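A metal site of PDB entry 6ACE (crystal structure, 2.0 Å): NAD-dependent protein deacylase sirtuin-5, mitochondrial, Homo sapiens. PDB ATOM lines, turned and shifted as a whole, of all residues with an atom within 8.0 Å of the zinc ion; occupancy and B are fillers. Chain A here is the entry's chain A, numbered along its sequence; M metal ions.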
ATOM      1  N   ARG A 130     -22.451  13.161 -20.604  1.00  0.00           N
ATOM      2  CA  ARG A 130     -21.768  14.010 -21.494  1.00  0.00           C
ATOM      3  C   ARG A 130     -22.757  14.882 -22.272  1.00  0.00           C
ATOM      4  O   ARG A 130     -23.738  14.383 -22.863  1.00  0.00           O
ATOM      5  CB  ARG A 130     -20.905  13.166 -22.438  1.00  0.00           C
ATOM      6  CG  ARG A 130     -20.143  14.004 -23.448  1.00  0.00           C
ATOM      7  CD  ARG A 130     -18.991  13.299 -24.111  1.00  0.00           C
ATOM      8  NE  ARG A 130     -19.385  12.408 -25.203  1.00  0.00           N
ATOM      9  CZ  ARG A 130     -19.459  11.067 -25.192  1.00  0.00           C
ATOM     10  NH1 ARG A 130     -19.292  10.336 -24.110  1.00  0.00           N
ATOM     11  NH2 ARG A 130     -19.785  10.413 -26.301  1.00  0.00           N
ATOM     12  N   CYS A 131     -22.468  16.169 -22.367  1.00  0.00           N
ATOM     13  CA  CYS A 131     -23.295  17.032 -23.251  1.00  0.00           C
ATOM     14  C   CYS A 131     -22.987  16.843 -24.722  1.00  0.00           C
ATOM     15  O   CYS A 131     -21.814  16.984 -25.166  1.00  0.00           O
ATOM     16  CB  CYS A 131     -23.145  18.502 -22.836  1.00  0.00           C
ATOM     17  SG  CYS A 131     -24.153  19.619 -23.803  1.00  0.00           S
ATOM     18  N   THR A 132     -24.023  16.503 -25.508  1.00  0.00           N
ATOM     19  CA  THR A 132     -23.885  16.344 -26.938  1.00  0.00           C
ATOM     20  C   THR A 132     -23.648  17.692 -27.682  1.00  0.00           C
ATOM     21  O   THR A 132     -23.448  17.661 -28.870  1.00  0.00           O
ATOM     22  CB  THR A 132     -25.167  15.705 -27.613  1.00  0.00           C
ATOM     23  OG1 THR A 132     -26.303  16.530 -27.373  1.00  0.00           O
ATOM     24  CG2 THR A 132     -25.446  14.299 -27.140  1.00  0.00           C
ATOM     25  N   SER A 133     -23.760  18.838 -27.024  1.00  0.00           N
ATOM     26  CA  SER A 133     -23.468  20.156 -27.637  1.00  0.00           C
ATOM     27  C   SER A 133     -22.058  20.668 -27.300  1.00  0.00           C
ATOM     28  O   SER A 133     -21.269  20.949 -28.187  1.00  0.00           O
ATOM     29  CB  SER A 133     -24.480  21.204 -27.174  1.00  0.00           C
ATOM     30  OG  SER A 133     -25.764  20.873 -27.701  1.00  0.00           O
ATOM     31  N   CYS A 134     -21.738  20.750 -26.024  1.00  0.00           N
ATOM     32  CA  CYS A 134     -20.436  21.257 -25.597  1.00  0.00           C
ATOM     33  C   CYS A 134     -19.402  20.214 -25.228  1.00  0.00           C
ATOM     34  O   CYS A 134     -18.261  20.576 -25.025  1.00  0.00           O
ATOM     35  CB  CYS A 134     -20.609  22.252 -24.450  1.00  0.00           C
ATOM     36  SG  CYS A 134     -21.096  21.586 -22.862  1.00  0.00           S
ATOM     37  N   GLY A 135     -19.782  18.937 -25.074  1.00  0.00           N
ATOM     38  CA  GLY A 135     -18.843  17.883 -24.675  1.00  0.00           C
ATOM     39  C   GLY A 135     -18.426  17.790 -23.216  1.00  0.00           C
ATOM     40  O   GLY A 135     -17.618  16.937 -22.866  1.00  0.00           O
ATOM     41  N   VAL A 136     -18.946  18.613 -22.343  1.00  0.00           N
ATOM     42  CA  VAL A 136     -18.552  18.485 -20.941  1.00  0.00           C
ATOM     43  C   VAL A 136     -19.074  17.166 -20.336  1.00  0.00           C
ATOM     44  O   VAL A 136     -20.227  16.746 -20.574  1.00  0.00           O
ATOM     45  CB  VAL A 136     -18.956  19.705 -20.124  1.00  0.00           C
ATOM     46  CG1 VAL A 136     -20.447  19.813 -19.976  1.00  0.00           C
ATOM     47  CG2 VAL A 136     -18.310  19.680 -18.716  1.00  0.00           C
ATOM     48  N   VAL A 137     -18.189  16.522 -19.580  1.00  0.00           N
ATOM     49  CA  VAL A 137     -18.485  15.288 -18.877  1.00  0.00           C
ATOM     50  C   VAL A 137     -18.712  15.650 -17.423  1.00  0.00           C
ATOM     51  O   VAL A 137     -17.873  16.301 -16.863  1.00  0.00           O
ATOM     52  CB  VAL A 137     -17.303  14.276 -18.964  1.00  0.00           C
ATOM     53  CG1 VAL A 137     -17.630  12.978 -18.236  1.00  0.00           C
ATOM     54  CG2 VAL A 137     -16.945  13.995 -20.425  1.00  0.00           C
ATOM     55  N   ARG A 171     -30.720  17.923 -19.574  1.00  0.00           N
ATOM     56  CA  ARG A 171     -30.115  19.001 -20.341  1.00  0.00           C
ATOM     57  C   ARG A 171     -28.890  19.535 -19.653  1.00  0.00           C
ATOM     58  O   ARG A 171     -28.834  19.627 -18.426  1.00  0.00           O
ATOM     59  CB  ARG A 171     -31.017  20.238 -20.544  1.00  0.00           C
ATOM     60  CG  ARG A 171     -32.396  20.008 -21.092  1.00  0.00           C
ATOM     61  CD  ARG A 171     -32.464  19.365 -22.471  1.00  0.00           C
ATOM     62  NE  ARG A 171     -31.826  20.109 -23.579  1.00  0.00           N
ATOM     63  CZ  ARG A 171     -32.057  19.856 -24.876  1.00  0.00           C
ATOM     64  NH1 ARG A 171     -32.930  18.909 -25.269  1.00  0.00           N
ATOM     65  NH2 ARG A 171     -31.402  20.535 -25.805  1.00  0.00           N
ATOM     66  N   CYS A 172     -27.958  19.996 -20.456  1.00  0.00           N
ATOM     67  CA  CYS A 172     -26.770  20.558 -19.947  1.00  0.00           C
ATOM     68  C   CYS A 172     -27.087  21.794 -19.075  1.00  0.00           C
ATOM     69  O   CYS A 172     -27.890  22.611 -19.470  1.00  0.00           O
ATOM     70  CB  CYS A 172     -25.922  20.959 -21.094  1.00  0.00           C
ATOM     71  SG  CYS A 172     -24.283  21.441 -20.585  1.00  0.00           S
ATOM     72  N   GLU A 173     -26.456  21.898 -17.916  1.00  0.00           N
ATOM     73  CA  GLU A 173     -26.620  23.090 -17.024  1.00  0.00           C
ATOM     74  C   GLU A 173     -25.439  24.100 -17.071  1.00  0.00           C
ATOM     75  O   GLU A 173     -25.351  25.007 -16.236  1.00  0.00           O
ATOM     76  CB  GLU A 173     -26.860  22.602 -15.617  1.00  0.00           C
ATOM     77  CG  GLU A 173     -28.082  21.671 -15.596  1.00  0.00           C
ATOM     78  CD  GLU A 173     -28.646  21.444 -14.223  1.00  0.00           C
ATOM     79  OE1 GLU A 173     -27.888  21.574 -13.261  1.00  0.00           O
ATOM     80  OE2 GLU A 173     -29.846  21.083 -14.095  1.00  0.00           O
ATOM     81  N   GLU A 174     -24.558  23.950 -18.050  1.00  0.00           N
ATOM     82  CA  GLU A 174     -23.503  24.925 -18.276  1.00  0.00           C
ATOM     83  C   GLU A 174     -24.191  26.180 -18.827  1.00  0.00           C
ATOM     84  O   GLU A 174     -24.971  26.102 -19.777  1.00  0.00           O
ATOM     85  CB  GLU A 174     -22.505  24.410 -19.295  1.00  0.00           C
ATOM     86  CG  GLU A 174     -21.829  23.105 -18.916  1.00  0.00           C
ATOM     87  CD  GLU A 174     -20.778  23.283 -17.851  1.00  0.00           C
ATOM     88  OE1 GLU A 174     -19.682  23.766 -18.187  1.00  0.00           O
ATOM     89  OE2 GLU A 174     -21.028  22.930 -16.682  1.00  0.00           O
ATOM     90  N   ALA A 175     -23.880  27.326 -18.232  1.00  0.00           N
ATOM     91  CA  ALA A 175     -24.548  28.554 -18.589  1.00  0.00           C
ATOM     92  C   ALA A 175     -24.616  28.727 -20.142  1.00  0.00           C
ATOM     93  O   ALA A 175     -23.606  28.675 -20.854  1.00  0.00           O
ATOM     94  CB  ALA A 175     -23.886  29.748 -17.900  1.00  0.00           C
ATOM     95  N   GLY A 176     -25.839  28.831 -20.669  1.00  0.00           N
ATOM     96  CA  GLY A 176     -26.019  29.116 -22.106  1.00  0.00           C
ATOM     97  C   GLY A 176     -25.733  27.961 -23.033  1.00  0.00           C
ATOM     98  O   GLY A 176     -25.828  28.110 -24.257  1.00  0.00           O
ATOM     99  N   CYS A 177     -25.443  26.774 -22.491  1.00  0.00           N
ATOM    100  CA  CYS A 177     -25.369  25.632 -23.367  1.00  0.00           C
ATOM    101  C   CYS A 177     -26.793  25.128 -23.702  1.00  0.00           C
ATOM    102  O   CYS A 177     -27.204  25.217 -24.824  1.00  0.00           O
ATOM    103  CB  CYS A 177     -24.509  24.492 -22.815  1.00  0.00           C
ATOM    104  SG  CYS A 177     -24.541  23.166 -24.004  1.00  0.00           S
ATOM    105  N   GLY A 178     -27.508  24.580 -22.730  1.00  0.00           N
ATOM    106  CA  GLY A 178     -28.846  24.004 -22.954  1.00  0.00           C
ATOM    107  C   GLY A 178     -28.890  22.653 -23.663  1.00  0.00           C
ATOM    108  O   GLY A 178     -29.987  22.129 -23.897  1.00  0.00           O
ATOM    109  N   GLY A 179     -27.725  22.070 -24.005  1.00  0.00           N
ATOM    110  CA  GLY A 179     -27.653  20.897 -24.874  1.00  0.00           C
ATOM    111  C   GLY A 179     -28.312  19.654 -24.302  1.00  0.00           C
ATOM    112  O   GLY A 179     -28.651  19.561 -23.133  1.00  0.00           O
ATOM    113  N   LEU A 180     -28.594  18.718 -25.158  1.00  0.00           N
ATOM    114  CA  LEU A 180     -29.176  17.440 -24.678  1.00  0.00           C
ATOM    115  C   LEU A 180     -28.063  16.581 -24.107  1.00  0.00           C
ATOM    116  O   LEU A 180     -27.016  16.451 -24.752  1.00  0.00           O
ATOM    117  CB  LEU A 180     -29.852  16.707 -25.818  1.00  0.00           C
ATOM    118  CG  LEU A 180     -30.288  15.282 -25.519  1.00  0.00           C
ATOM    119  CD1 LEU A 180     -31.341  15.278 -24.433  1.00  0.00           C
ATOM    120  CD2 LEU A 180     -30.767  14.657 -26.823  1.00  0.00           C
ATOM    121  N   LEU A 181     -28.293  16.014 -22.911  1.00  0.00           N
ATOM    122  CA  LEU A 181     -27.270  15.147 -22.332  1.00  0.00           C
ATOM    123  C   LEU A 181     -27.451  13.702 -22.811  1.00  0.00           C
ATOM    124  O   LEU A 181     -28.537  13.278 -23.141  1.00  0.00           O
ATOM    125  CB  LEU A 181     -27.273  15.223 -20.792  1.00  0.00           C
ATOM    126  CG  LEU A 181     -27.086  16.552 -20.149  1.00  0.00           C
ATOM    127  CD1 LEU A 181     -27.206  16.474 -18.600  1.00  0.00           C
ATOM    128  CD2 LEU A 181     -25.730  17.109 -20.570  1.00  0.00           C
HETATM  129 ZN    ZN M   1     -23.456  21.538 -22.715  1.00  0.00          ZN
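Within 4 Å of the zinc ion: Cys 131, Cys 134, Cys 172 and Cys 177.
The side-chain sulfur of Cys 177 sits close to the backbone NH of Gly 179, 3.4 Å away.
The backbone NH (N) of Glu 174 sits close to the side-chain sulfur (SG) of Cys 172, at 3.6 Å.
The side-chain sulfur (SG) of Cys 134 lies close to the backbone NH (N) of Val 136 (3.7 Å).
The backbone carbonyl oxygen (O) of Gly 179 is in hydrogen-bond range of the backbone NH (N) of Cys 172 (2.8 Å).
O of Val 136 is in hydrogen-bond range of N of Cys 131 (2.9 Å).
The side-chain sulfur (SG) of Cys 131 sits close to the backbone NH (N) of Ser 133, 3.3 Å away.
The zinc ion is bound by the side-chain sulfur of Cys 172 (2.3 Å), the side-chain sulfur of Cys 131 (2.3 Å), the side-chain sulfur of Cys 177 (2.3 Å) and the side-chain sulfur of Cys 134 (2.4 Å).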
